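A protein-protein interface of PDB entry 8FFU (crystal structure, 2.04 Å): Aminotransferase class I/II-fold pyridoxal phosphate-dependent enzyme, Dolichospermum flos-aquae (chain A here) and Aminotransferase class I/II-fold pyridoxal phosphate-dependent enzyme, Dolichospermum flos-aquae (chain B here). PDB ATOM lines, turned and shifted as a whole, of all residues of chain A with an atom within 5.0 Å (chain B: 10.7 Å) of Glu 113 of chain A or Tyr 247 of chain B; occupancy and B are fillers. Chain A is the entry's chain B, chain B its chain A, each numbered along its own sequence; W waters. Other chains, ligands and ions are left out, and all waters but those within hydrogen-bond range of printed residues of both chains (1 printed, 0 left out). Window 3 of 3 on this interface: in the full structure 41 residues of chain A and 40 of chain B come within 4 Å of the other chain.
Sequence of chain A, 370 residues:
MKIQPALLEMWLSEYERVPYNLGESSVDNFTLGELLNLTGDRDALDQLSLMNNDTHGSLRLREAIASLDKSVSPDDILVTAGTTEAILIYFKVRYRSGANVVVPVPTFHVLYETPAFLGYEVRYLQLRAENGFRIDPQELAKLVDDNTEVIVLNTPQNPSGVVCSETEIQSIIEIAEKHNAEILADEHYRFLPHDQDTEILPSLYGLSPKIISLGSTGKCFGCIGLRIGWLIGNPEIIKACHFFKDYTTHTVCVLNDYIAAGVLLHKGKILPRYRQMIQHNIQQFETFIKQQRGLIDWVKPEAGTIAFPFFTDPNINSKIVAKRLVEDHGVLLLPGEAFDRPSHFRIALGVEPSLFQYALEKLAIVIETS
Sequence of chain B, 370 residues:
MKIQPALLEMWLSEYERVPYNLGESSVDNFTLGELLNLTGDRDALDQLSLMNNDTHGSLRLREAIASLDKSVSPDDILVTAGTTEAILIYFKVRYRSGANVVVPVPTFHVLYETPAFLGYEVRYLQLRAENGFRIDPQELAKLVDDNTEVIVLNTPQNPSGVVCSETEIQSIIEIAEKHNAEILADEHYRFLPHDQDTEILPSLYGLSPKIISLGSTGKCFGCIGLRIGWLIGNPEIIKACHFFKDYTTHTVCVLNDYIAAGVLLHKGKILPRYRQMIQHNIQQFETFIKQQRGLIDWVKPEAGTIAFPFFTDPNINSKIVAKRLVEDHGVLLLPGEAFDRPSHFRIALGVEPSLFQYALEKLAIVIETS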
ATOM      1  N   THR A  84     -10.724 -23.668 -37.010  1.00  0.00           N
ATOM      2  CA  THR A  84     -10.377 -23.901 -35.613  1.00  0.00           C
ATOM      3  C   THR A  84     -10.628 -25.352 -35.226  1.00  0.00           C
ATOM      4  O   THR A  84      -9.793 -25.981 -34.563  1.00  0.00           O
ATOM      5  CB  THR A  84     -11.181 -22.963 -34.706  1.00  0.00           C
ATOM      6  OG1 THR A  84     -10.953 -21.602 -35.085  1.00  0.00           O
ATOM      7  CG2 THR A  84     -10.783 -23.153 -33.256  1.00  0.00           C
ATOM      8  N   LEU A  88      -7.870 -28.347 -34.460  1.00  0.00           N
ATOM      9  CA  LEU A  88      -7.946 -29.135 -33.236  1.00  0.00           C
ATOM     10  C   LEU A  88      -7.925 -30.627 -33.535  1.00  0.00           C
ATOM     11  O   LEU A  88      -7.184 -31.390 -32.903  1.00  0.00           O
ATOM     12  CB  LEU A  88      -9.203 -28.759 -32.456  1.00  0.00           C
ATOM     13  CG  LEU A  88      -9.469 -29.602 -31.212  1.00  0.00           C
ATOM     14  CD1 LEU A  88      -8.329 -29.440 -30.233  1.00  0.00           C
ATOM     15  CD2 LEU A  88     -10.788 -29.193 -30.571  1.00  0.00           C
ATOM     16  N   HIS A 109      -2.773 -17.358 -33.392  1.00  0.00           N
ATOM     17  CA  HIS A 109      -2.321 -17.958 -32.135  1.00  0.00           C
ATOM     18  C   HIS A 109      -2.741 -19.420 -31.988  1.00  0.00           C
ATOM     19  O   HIS A 109      -2.036 -20.200 -31.337  1.00  0.00           O
ATOM     20  CB  HIS A 109      -2.830 -17.139 -30.948  1.00  0.00           C
ATOM     21  CG  HIS A 109      -4.323 -17.115 -30.819  1.00  0.00           C
ATOM     22  ND1 HIS A 109      -4.999 -17.837 -29.857  1.00  0.00           N
ATOM     23  CD2 HIS A 109      -5.271 -16.460 -31.532  1.00  0.00           C
ATOM     24  CE1 HIS A 109      -6.298 -17.626 -29.982  1.00  0.00           C
ATOM     25  NE2 HIS A 109      -6.489 -16.794 -30.991  1.00  0.00           N
ATOM     26  N   VAL A 110      -3.872 -19.815 -32.576  1.00  0.00           N
ATOM     27  CA  VAL A 110      -4.334 -21.196 -32.441  1.00  0.00           C
ATOM     28  C   VAL A 110      -3.334 -22.169 -33.052  1.00  0.00           C
ATOM     29  O   VAL A 110      -3.188 -23.303 -32.577  1.00  0.00           O
ATOM     30  CB  VAL A 110      -5.735 -21.350 -33.076  1.00  0.00           C
ATOM     31  CG1 VAL A 110      -6.092 -22.818 -33.275  1.00  0.00           C
ATOM     32  CG2 VAL A 110      -6.790 -20.649 -32.232  1.00  0.00           C
ATOM     33  N   LEU A 111      -2.600 -21.734 -34.081  1.00  0.00           N
ATOM     34  CA  LEU A 111      -1.698 -22.636 -34.793  1.00  0.00           C
ATOM     35  C   LEU A 111      -0.571 -23.151 -33.904  1.00  0.00           C
ATOM     36  O   LEU A 111      -0.022 -24.224 -34.167  1.00  0.00           O
ATOM     37  CB  LEU A 111      -1.136 -21.940 -36.027  1.00  0.00           C
ATOM     38  CG  LEU A 111      -2.187 -21.764 -37.124  1.00  0.00           C
ATOM     39  CD1 LEU A 111      -1.714 -20.813 -38.202  1.00  0.00           C
ATOM     40  CD2 LEU A 111      -2.554 -23.110 -37.727  1.00  0.00           C
ATOM     41  N   TYR A 112      -0.203 -22.414 -32.859  1.00  0.00           N
ATOM     42  CA  TYR A 112       0.754 -22.929 -31.894  1.00  0.00           C
ATOM     43  C   TYR A 112       0.165 -23.178 -30.515  1.00  0.00           C
ATOM     44  O   TYR A 112       0.740 -23.962 -29.754  1.00  0.00           O
ATOM     45  CB  TYR A 112       1.960 -21.983 -31.764  1.00  0.00           C
ATOM     46  CG  TYR A 112       1.621 -20.545 -31.444  1.00  0.00           C
ATOM     47  CD1 TYR A 112       1.394 -19.625 -32.460  1.00  0.00           C
ATOM     48  CD2 TYR A 112       1.555 -20.102 -30.131  1.00  0.00           C
ATOM     49  CE1 TYR A 112       1.093 -18.308 -32.175  1.00  0.00           C
ATOM     50  CE2 TYR A 112       1.254 -18.789 -29.839  1.00  0.00           C
ATOM     51  CZ  TYR A 112       1.025 -17.895 -30.866  1.00  0.00           C
ATOM     52  OH  TYR A 112       0.721 -16.584 -30.584  1.00  0.00           O
ATOM     53  N   GLU A 113      -0.976 -22.570 -30.184  1.00  0.00           N
ATOM     54  CA  GLU A 113      -1.533 -22.752 -28.847  1.00  0.00           C
ATOM     55  C   GLU A 113      -2.282 -24.070 -28.717  1.00  0.00           C
ATOM     56  O   GLU A 113      -2.154 -24.755 -27.698  1.00  0.00           O
ATOM     57  CB  GLU A 113      -2.456 -21.587 -28.503  1.00  0.00           C
ATOM     58  CG  GLU A 113      -1.711 -20.329 -28.125  1.00  0.00           C
ATOM     59  CD  GLU A 113      -2.638 -19.207 -27.725  1.00  0.00           C
ATOM     60  OE1 GLU A 113      -3.789 -19.179 -28.213  1.00  0.00           O
ATOM     61  OE2 GLU A 113      -2.211 -18.346 -26.932  1.00  0.00           O
ATOM     62  N   THR A 114      -3.059 -24.444 -29.731  1.00  0.00           N
ATOM     63  CA  THR A 114      -3.725 -25.745 -29.704  1.00  0.00           C
ATOM     64  C   THR A 114      -2.737 -26.903 -29.604  1.00  0.00           C
ATOM     65  O   THR A 114      -2.976 -27.813 -28.793  1.00  0.00           O
ATOM     66  CB  THR A 114      -4.655 -25.878 -30.915  1.00  0.00           C
ATOM     67  OG1 THR A 114      -5.770 -24.995 -30.749  1.00  0.00           O
ATOM     68  CG2 THR A 114      -5.162 -27.304 -31.049  1.00  0.00           C
ATOM     69  N   PRO A 115      -1.639 -26.953 -30.370  1.00  0.00           N
ATOM     70  CA  PRO A 115      -0.661 -28.029 -30.133  1.00  0.00           C
ATOM     71  C   PRO A 115      -0.062 -27.990 -28.739  1.00  0.00           C
ATOM     72  O   PRO A 115       0.297 -29.045 -28.199  1.00  0.00           O
ATOM     73  CB  PRO A 115       0.405 -27.782 -31.211  1.00  0.00           C
ATOM     74  CG  PRO A 115      -0.291 -27.024 -32.260  1.00  0.00           C
ATOM     75  CD  PRO A 115      -1.277 -26.152 -31.552  1.00  0.00           C
ATOM     76  N   ALA A 116       0.074 -26.803 -28.141  1.00  0.00           N
ATOM     77  CA  ALA A 116       0.598 -26.727 -26.782  1.00  0.00           C
ATOM     78  C   ALA A 116      -0.378 -27.332 -25.781  1.00  0.00           C
ATOM     79  O   ALA A 116       0.035 -28.058 -24.871  1.00  0.00           O
ATOM     80  CB  ALA A 116       0.915 -25.278 -26.420  1.00  0.00           C
ATOM     81  N   PHE A 117      -1.676 -27.055 -25.934  1.00  0.00           N
ATOM     82  CA  PHE A 117      -2.664 -27.695 -25.069  1.00  0.00           C
ATOM     83  C   PHE A 117      -2.655 -29.205 -25.235  1.00  0.00           C
ATOM     84  O   PHE A 117      -2.858 -29.936 -24.260  1.00  0.00           O
ATOM     85  CB  PHE A 117      -4.064 -27.146 -25.348  1.00  0.00           C
ATOM     86  CG  PHE A 117      -4.279 -25.747 -24.855  1.00  0.00           C
ATOM     87  CD1 PHE A 117      -3.679 -25.312 -23.684  1.00  0.00           C
ATOM     88  CD2 PHE A 117      -5.074 -24.863 -25.563  1.00  0.00           C
ATOM     89  CE1 PHE A 117      -3.874 -24.021 -23.223  1.00  0.00           C
ATOM     90  CE2 PHE A 117      -5.267 -23.570 -25.109  1.00  0.00           C
ATOM     91  CZ  PHE A 117      -4.666 -23.150 -23.936  1.00  0.00           C
ATOM     92  N   THR B  55     -19.691 -14.637 -28.030  1.00  0.00           N
ATOM     93  CA  THR B  55     -18.933 -15.859 -27.784  1.00  0.00           C
ATOM     94  C   THR B  55     -19.512 -16.695 -26.648  1.00  0.00           C
ATOM     95  O   THR B  55     -19.037 -17.814 -26.417  1.00  0.00           O
ATOM     96  CB  THR B  55     -17.463 -15.525 -27.512  1.00  0.00           C
ATOM     97  OG1 THR B  55     -17.365 -14.590 -26.431  1.00  0.00           O
ATOM     98  CG2 THR B  55     -16.829 -14.919 -28.753  1.00  0.00           C
ATOM     99  N   LEU B  78     -23.373 -21.049 -21.317  1.00  0.00           N
ATOM    100  CA  LEU B  78     -22.416 -20.983 -22.419  1.00  0.00           C
ATOM    101  C   LEU B  78     -22.939 -21.855 -23.552  1.00  0.00           C
ATOM    102  O   LEU B  78     -22.901 -23.084 -23.456  1.00  0.00           O
ATOM    103  CB  LEU B  78     -21.029 -21.441 -21.975  1.00  0.00           C
ATOM    104  CG  LEU B  78     -19.905 -21.384 -23.011  1.00  0.00           C
ATOM    105  CD1 LEU B  78     -19.516 -19.950 -23.324  1.00  0.00           C
ATOM    106  CD2 LEU B  78     -18.703 -22.170 -22.517  1.00  0.00           C
ATOM    107  N   GLU B  85     -19.701 -30.644 -28.047  1.00  0.00           N
ATOM    108  CA  GLU B  85     -18.632 -29.684 -27.781  1.00  0.00           C
ATOM    109  C   GLU B  85     -18.561 -29.337 -26.299  1.00  0.00           C
ATOM    110  O   GLU B  85     -17.468 -29.226 -25.734  1.00  0.00           O
ATOM    111  CB  GLU B  85     -18.832 -28.415 -28.618  1.00  0.00           C
ATOM    112  CG  GLU B  85     -17.706 -27.395 -28.479  1.00  0.00           C
ATOM    113  CD  GLU B  85     -17.967 -26.093 -29.226  1.00  0.00           C
ATOM    114  OE1 GLU B  85     -19.132 -25.652 -29.288  1.00  0.00           O
ATOM    115  OE2 GLU B  85     -16.998 -25.500 -29.751  1.00  0.00           O
ATOM    116  N   LEU B  88     -16.752 -31.922 -24.344  1.00  0.00           N
ATOM    117  CA  LEU B  88     -15.316 -31.893 -24.614  1.00  0.00           C
ATOM    118  C   LEU B  88     -14.619 -30.790 -23.828  1.00  0.00           C
ATOM    119  O   LEU B  88     -13.589 -31.025 -23.184  1.00  0.00           O
ATOM    120  CB  LEU B  88     -15.077 -31.710 -26.111  1.00  0.00           C
ATOM    121  CG  LEU B  88     -13.626 -31.539 -26.549  1.00  0.00           C
ATOM    122  CD1 LEU B  88     -12.821 -32.778 -26.206  1.00  0.00           C
ATOM    123  CD2 LEU B  88     -13.568 -31.245 -28.039  1.00  0.00           C
ATOM    124  N   ILE B  89     -15.162 -29.571 -23.874  1.00  0.00           N
ATOM    125  CA  ILE B  89     -14.511 -28.453 -23.200  1.00  0.00           C
ATOM    126  C   ILE B  89     -14.567 -28.635 -21.689  1.00  0.00           C
ATOM    127  O   ILE B  89     -13.592 -28.346 -20.982  1.00  0.00           O
ATOM    128  CB  ILE B  89     -15.127 -27.114 -23.646  1.00  0.00           C
ATOM    129  CG1 ILE B  89     -16.612 -27.037 -23.294  1.00  0.00           C
ATOM    130  CG2 ILE B  89     -14.936 -26.915 -25.141  1.00  0.00           C
ATOM    131  CD1 ILE B  89     -17.254 -25.723 -23.653  1.00  0.00           C
ATOM    132  N   LYS B  92     -12.030 -31.184 -20.606  1.00  0.00           N
ATOM    133  CA  LYS B  92     -10.692 -30.629 -20.783  1.00  0.00           C
ATOM    134  C   LYS B  92     -10.340 -29.725 -19.611  1.00  0.00           C
ATOM    135  O   LYS B  92      -9.278 -29.869 -18.996  1.00  0.00           O
ATOM    136  CB  LYS B  92     -10.604 -29.873 -22.113  1.00  0.00           C
ATOM    137  CG  LYS B  92      -9.297 -29.114 -22.331  1.00  0.00           C
ATOM    138  CD  LYS B  92      -8.077 -30.024 -22.395  1.00  0.00           C
ATOM    139  CE  LYS B  92      -6.795 -29.201 -22.515  1.00  0.00           C
ATOM    140  NZ  LYS B  92      -5.552 -30.021 -22.461  1.00  0.00           N
ATOM    141  N   VAL B  93     -11.256 -28.826 -19.249  1.00  0.00           N
ATOM    142  CA  VAL B  93     -10.995 -27.862 -18.186  1.00  0.00           C
ATOM    143  C   VAL B  93     -10.806 -28.552 -16.838  1.00  0.00           C
ATOM    144  O   VAL B  93      -9.998 -28.106 -16.014  1.00  0.00           O
ATOM    145  CB  VAL B  93     -12.142 -26.833 -18.142  1.00  0.00           C
ATOM    146  CG1 VAL B  93     -12.106 -26.044 -16.847  1.00  0.00           C
ATOM    147  CG2 VAL B  93     -12.067 -25.905 -19.347  1.00  0.00           C
ATOM    148  N   LYS B 239     -16.164 -19.296 -17.226  1.00  0.00           N
ATOM    149  CA  LYS B 239     -15.006 -18.579 -17.753  1.00  0.00           C
ATOM    150  C   LYS B 239     -13.966 -19.547 -18.294  1.00  0.00           C
ATOM    151  O   LYS B 239     -13.355 -19.298 -19.342  1.00  0.00           O
ATOM    152  CB  LYS B 239     -14.390 -17.705 -16.661  1.00  0.00           C
ATOM    153  CG  LYS B 239     -13.235 -16.843 -17.140  1.00  0.00           C
ATOM    154  CD  LYS B 239     -12.415 -16.285 -15.983  1.00  0.00           C
ATOM    155  CE  LYS B 239     -11.874 -17.402 -15.092  1.00  0.00           C
ATOM    156  NZ  LYS B 239     -11.146 -18.453 -15.871  1.00  0.00           N
ATOM    157  N   ALA B 240     -13.761 -20.666 -17.602  1.00  0.00           N
ATOM    158  CA  ALA B 240     -12.754 -21.620 -18.041  1.00  0.00           C
ATOM    159  C   ALA B 240     -13.196 -22.351 -19.302  1.00  0.00           C
ATOM    160  O   ALA B 240     -12.370 -22.648 -20.172  1.00  0.00           O
ATOM    161  CB  ALA B 240     -12.448 -22.604 -16.919  1.00  0.00           C
ATOM    162  N   CYS B 241     -14.484 -22.676 -19.412  1.00  0.00           N
ATOM    163  CA  CYS B 241     -14.963 -23.332 -20.624  1.00  0.00           C
ATOM    164  C   CYS B 241     -15.017 -22.351 -21.787  1.00  0.00           C
ATOM    165  O   CYS B 241     -14.710 -22.715 -22.927  1.00  0.00           O
ATOM    166  CB  CYS B 241     -16.333 -23.964 -20.383  1.00  0.00           C
ATOM    167  SG  CYS B 241     -16.285 -25.437 -19.342  1.00  0.00           S
ATOM    168  N   HIS B 242     -15.417 -21.107 -21.516  1.00  0.00           N
ATOM    169  CA  HIS B 242     -15.442 -20.086 -22.559  1.00  0.00           C
ATOM    170  C   HIS B 242     -14.047 -19.827 -23.109  1.00  0.00           C
ATOM    171  O   HIS B 242     -13.878 -19.593 -24.310  1.00  0.00           O
ATOM    172  CB  HIS B 242     -16.051 -18.795 -22.013  1.00  0.00           C
ATOM    173  CG  HIS B 242     -16.022 -17.650 -22.978  1.00  0.00           C
ATOM    174  ND1 HIS B 242     -15.064 -16.661 -22.928  1.00  0.00           N
ATOM    175  CD2 HIS B 242     -16.838 -17.332 -24.012  1.00  0.00           C
ATOM    176  CE1 HIS B 242     -15.291 -15.782 -23.888  1.00  0.00           C
ATOM    177  NE2 HIS B 242     -16.362 -16.165 -24.559  1.00  0.00           N
ATOM    178  N   PHE B 243     -13.034 -19.860 -22.243  1.00  0.00           N
ATOM    179  CA  PHE B 243     -11.669 -19.655 -22.706  1.00  0.00           C
ATOM    180  C   PHE B 243     -11.251 -20.752 -23.679  1.00  0.00           C
ATOM    181  O   PHE B 243     -10.695 -20.474 -24.747  1.00  0.00           O
ATOM    182  CB  PHE B 243     -10.706 -19.589 -21.523  1.00  0.00           C
ATOM    183  CG  PHE B 243      -9.278 -19.800 -21.913  1.00  0.00           C
ATOM    184  CD1 PHE B 243      -8.551 -18.767 -22.481  1.00  0.00           C
ATOM    185  CD2 PHE B 243      -8.669 -21.029 -21.742  1.00  0.00           C
ATOM    186  CE1 PHE B 243      -7.236 -18.947 -22.858  1.00  0.00           C
ATOM    187  CE2 PHE B 243      -7.357 -21.221 -22.117  1.00  0.00           C
ATOM    188  CZ  PHE B 243      -6.637 -20.176 -22.678  1.00  0.00           C
ATOM    189  N   PHE B 244     -11.499 -22.014 -23.322  1.00  0.00           N
ATOM    190  CA  PHE B 244     -11.017 -23.104 -24.159  1.00  0.00           C
ATOM    191  C   PHE B 244     -11.852 -23.318 -25.414  1.00  0.00           C
ATOM    192  O   PHE B 244     -11.351 -23.927 -26.366  1.00  0.00           O
ATOM    193  CB  PHE B 244     -10.960 -24.409 -23.363  1.00  0.00           C
ATOM    194  CG  PHE B 244     -10.361 -25.549 -24.132  1.00  0.00           C
ATOM    195  CD1 PHE B 244      -8.989 -25.639 -24.311  1.00  0.00           C
ATOM    196  CD2 PHE B 244     -11.173 -26.519 -24.704  1.00  0.00           C
ATOM    197  CE1 PHE B 244      -8.434 -26.683 -25.037  1.00  0.00           C
ATOM    198  CE2 PHE B 244     -10.627 -27.565 -25.425  1.00  0.00           C
ATOM    199  CZ  PHE B 244      -9.253 -27.648 -25.593  1.00  0.00           C
ATOM    200  N   LYS B 245     -13.091 -22.820 -25.463  1.00  0.00           N
ATOM    201  CA  LYS B 245     -13.874 -22.944 -26.689  1.00  0.00           C
ATOM    202  C   LYS B 245     -13.258 -22.150 -27.835  1.00  0.00           C
ATOM    203  O   LYS B 245     -13.566 -22.418 -29.004  1.00  0.00           O
ATOM    204  CB  LYS B 245     -15.318 -22.501 -26.449  1.00  0.00           C
ATOM    205  CG  LYS B 245     -16.266 -22.791 -27.609  1.00  0.00           C
ATOM    206  CD  LYS B 245     -17.710 -22.576 -27.216  1.00  0.00           C
ATOM    207  CE  LYS B 245     -17.933 -21.181 -26.660  1.00  0.00           C
ATOM    208  NZ  LYS B 245     -18.129 -20.169 -27.736  1.00  0.00           N
ATOM    209  N   ASP B 246     -12.388 -21.185 -27.522  1.00  0.00           N
ATOM    210  CA  ASP B 246     -11.644 -20.465 -28.548  1.00  0.00           C
ATOM    211  C   ASP B 246     -10.795 -21.408 -29.388  1.00  0.00           C
ATOM    212  O   ASP B 246     -10.446 -21.074 -30.526  1.00  0.00           O
ATOM    213  CB  ASP B 246     -10.761 -19.409 -27.882  1.00  0.00           C
ATOM    214  CG  ASP B 246     -10.557 -18.184 -28.748  1.00  0.00           C
ATOM    215  OD1 ASP B 246     -10.408 -18.337 -29.981  1.00  0.00           O
ATOM    216  OD2 ASP B 246     -10.553 -17.064 -28.187  1.00  0.00           O
ATOM    217  N   TYR B 247     -10.454 -22.574 -28.843  1.00  0.00           N
ATOM    218  CA  TYR B 247      -9.613 -23.561 -29.503  1.00  0.00           C
ATOM    219  C   TYR B 247     -10.409 -24.760 -30.004  1.00  0.00           C
ATOM    220  O   TYR B 247      -9.814 -25.783 -30.356  1.00  0.00           O
ATOM    221  CB  TYR B 247      -8.501 -23.990 -28.547  1.00  0.00           C
ATOM    222  CG  TYR B 247      -7.846 -22.777 -27.929  1.00  0.00           C
ATOM    223  CD1 TYR B 247      -6.927 -22.015 -28.647  1.00  0.00           C
ATOM    224  CD2 TYR B 247      -8.189 -22.356 -26.650  1.00  0.00           C
ATOM    225  CE1 TYR B 247      -6.350 -20.889 -28.096  1.00  0.00           C
ATOM    226  CE2 TYR B 247      -7.618 -21.229 -26.091  1.00  0.00           C
ATOM    227  CZ  TYR B 247      -6.699 -20.500 -26.816  1.00  0.00           C
ATOM    228  OH  TYR B 247      -6.129 -19.380 -26.255  1.00  0.00           O
ATOM    229  N   THR B 248     -11.741 -24.668 -30.025  1.00  0.00           N
ATOM    230  CA  THR B 248     -12.578 -25.729 -30.583  1.00  0.00           C
ATOM    231  C   THR B 248     -13.365 -25.214 -31.782  1.00  0.00           C
ATOM    232  O   THR B 248     -13.100 -25.644 -32.906  1.00  0.00           O
ATOM    233  CB  THR B 248     -13.495 -26.328 -29.509  1.00  0.00           C
ATOM    234  OG1 THR B 248     -14.337 -25.310 -28.956  1.00  0.00           O
ATOM    235  CG2 THR B 248     -12.666 -26.942 -28.390  1.00  0.00           C
ATOM    236  N   THR B 249     -14.320 -24.302 -31.589  1.00  0.00           N
ATOM    237  CA  THR B 249     -15.056 -23.697 -32.695  1.00  0.00           C
ATOM    238  C   THR B 249     -15.196 -22.190 -32.560  1.00  0.00           C
ATOM    239  O   THR B 249     -15.743 -21.556 -33.474  1.00  0.00           O
ATOM    240  CB  THR B 249     -16.469 -24.299 -32.829  1.00  0.00           C
ATOM    241  OG1 THR B 249     -17.253 -23.957 -31.677  1.00  0.00           O
ATOM    242  CG2 THR B 249     -16.418 -25.817 -32.981  1.00  0.00           C
ATOM    243  N   HIS B 250     -14.745 -21.607 -31.447  1.00  0.00           N
ATOM    244  CA  HIS B 250     -14.806 -20.179 -31.162  1.00  0.00           C
ATOM    245  C   HIS B 250     -16.241 -19.696 -30.947  1.00  0.00           C
ATOM    246  O   HIS B 250     -16.585 -19.279 -29.837  1.00  0.00           O
ATOM    247  CB  HIS B 250     -14.097 -19.383 -32.265  1.00  0.00           C
ATOM    248  CG  HIS B 250     -13.976 -17.923 -31.968  1.00  0.00           C
ATOM    249  ND1 HIS B 250     -14.514 -16.949 -32.780  1.00  0.00           N
ATOM    250  CD2 HIS B 250     -13.400 -17.272 -30.929  1.00  0.00           C
ATOM    251  CE1 HIS B 250     -14.265 -15.761 -32.260  1.00  0.00           C
ATOM    252  NE2 HIS B 250     -13.591 -15.929 -31.137  1.00  0.00           N
ATOM    253  N   THR B 251     -17.087 -19.737 -31.980  1.00  0.00           N
ATOM    254  CA  THR B 251     -18.479 -19.309 -31.857  1.00  0.00           C
ATOM    255  C   THR B 251     -19.376 -20.261 -32.636  1.00  0.00           C
ATOM    256  O   THR B 251     -18.904 -21.068 -33.440  1.00  0.00           O
ATOM    257  CB  THR B 251     -18.714 -17.870 -32.372  1.00  0.00           C
ATOM    258  OG1 THR B 251     -18.320 -17.763 -33.746  1.00  0.00           O
ATOM    259  CG2 THR B 251     -17.943 -16.851 -31.551  1.00  0.00           C
HETATM  260  O   HOH W   1      -8.053 -25.518 -32.667  1.00  0.00           O
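Among the printed residues, pairs that only touch across the chains: Thr 84 of chain A with Asp 246 of chain B (3.4 Å), Thr 84 of chain A with Tyr 247 of chain B (3.6 Å), Thr 84 of chain A with Thr 248 of chain B (3.4 Å), Leu 88 of chain A with Tyr 247 of chain B (3.6 Å), Leu 88 of chain A with Thr 248 of chain B (3.7 Å), His 109 of chain A with Tyr 247 of chain B (3.8 Å), Val 110 of chain A with Tyr 247 of chain B (3.8 Å), Thr 114 of chain A with Tyr 247 of chain B (3.6 Å), Phe 117 of chain A with Phe 243 of chain B (3.8 Å), Phe 117 of chain A with Phe 244 of chain B (3.9 Å) and Phe 117 of chain A with Tyr 247 of chain B (3.5 Å).
The side-chain carboxylate of Glu 85 of chain B is in hydrogen-bond range of the side-chain hydroxyl of Thr 248 of chain B, at 2.8 Å. The backbone carbonyl oxygen of Lys 245 of chain B lies within hydrogen-bond range of the side-chain hydroxyl of Thr 248 of chain B (3.0 Å). OE1 of Glu 113 of chain A is in hydrogen-bond range of ND1 of His 109 of chain A (2.4 Å).
The backbone carbonyl oxygen (O) of Phe 117 of chain A lies within hydrogen-bond range of the side-chain amino group (NZ) of Lys 92 of chain B, at 3.2 Å. OH of Tyr 247 of chain B is in hydrogen-bond range of OE1 of Glu 113 of chain A (3.1 Å).
Water W1 lies within hydrogen-bond range of the backbone carbonyl oxygen of Thr 84 of chain A (2.6 Å), the backbone carbonyl oxygen of Tyr 247 of chain B (2.9 Å), the side-chain hydroxyl of Thr 114 of chain A (3.0 Å) and the backbone NH of Leu 88 of chain A (3.4 Å).
Glu 113 of chain A touches one residue of chain B. Tyr 247 of chain B touches seven residues of chain A. Val 110 of chain A touches just one residue of chain B: Tyr 247 (3.8 Å). No residue of chain B comes within 4 Å of Tyr 112 of chain A. Of chain B, only Tyr 247 comes within 4 Å of Thr 114 of chain A. No residue of chain B comes within 4 Å of Pro 115 of chain A. No residue of chain B comes within 4 Å of Ala 116 of chain A. Phe 117 of chain A touches just these residues of chain B: Lys 92, Phe 243, Phe 244 and Tyr 247. Printed residues of chain B within 4 Å of Leu 88 of chain A: Tyr 247 (3.6 Å) and Thr 248 (3.7 Å). Printed residues of chain A within 4 Å of Phe 244 of chain B: Phe 117. Of the printed residues of chain A, Phe 243 of chain B touches Phe 117. Printed residues of chain B within 4 Å of Thr 84 of chain A: Asp 246 (3.4 Å), Tyr 247 (3.6 Å) and Thr 248 (3.4 Å). Printed residues of chain A within 4 Å of Lys 92 of chain B: Phe 117. Cys 241 of chain B touches none of the printed residues of chain A. The nearest residue of chain B that does not touch Glu 113 of chain A is Phe 243 of chain B (6.3 Å). The nearest printed residue of chain A that does not touch Tyr 247 of chain B is Leu 111 of chain A (7.0 Å). The nearest printed residue of chain B that does not touch Leu 88 of chain A is Leu 88 of chain B (4.3 Å).
Printed residues of chain B that touch a printed residue of chain A: Lys 92, Phe 243, Phe 244, Asp 246, Tyr 247 and Thr 248. Hydrophobic or aromatic side chains of chain B that line the printed part of chain A: Phe 243, Phe 244 and Tyr 247. Hydrophobic or aromatic side chains of chain A within 4 Å of the printed part of chain B: Leu 88, His 109, Val 110 and Phe 117. Along chain A the printed residues that touch a printed residue of chain B span positions 84 to 117. Among the printed residues, 13 pairs touch across the chains. Among the printed residues, no Asp or Glu carboxylate lies within 4 Å of a Lys or Arg side-chain nitrogen of the other chain.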
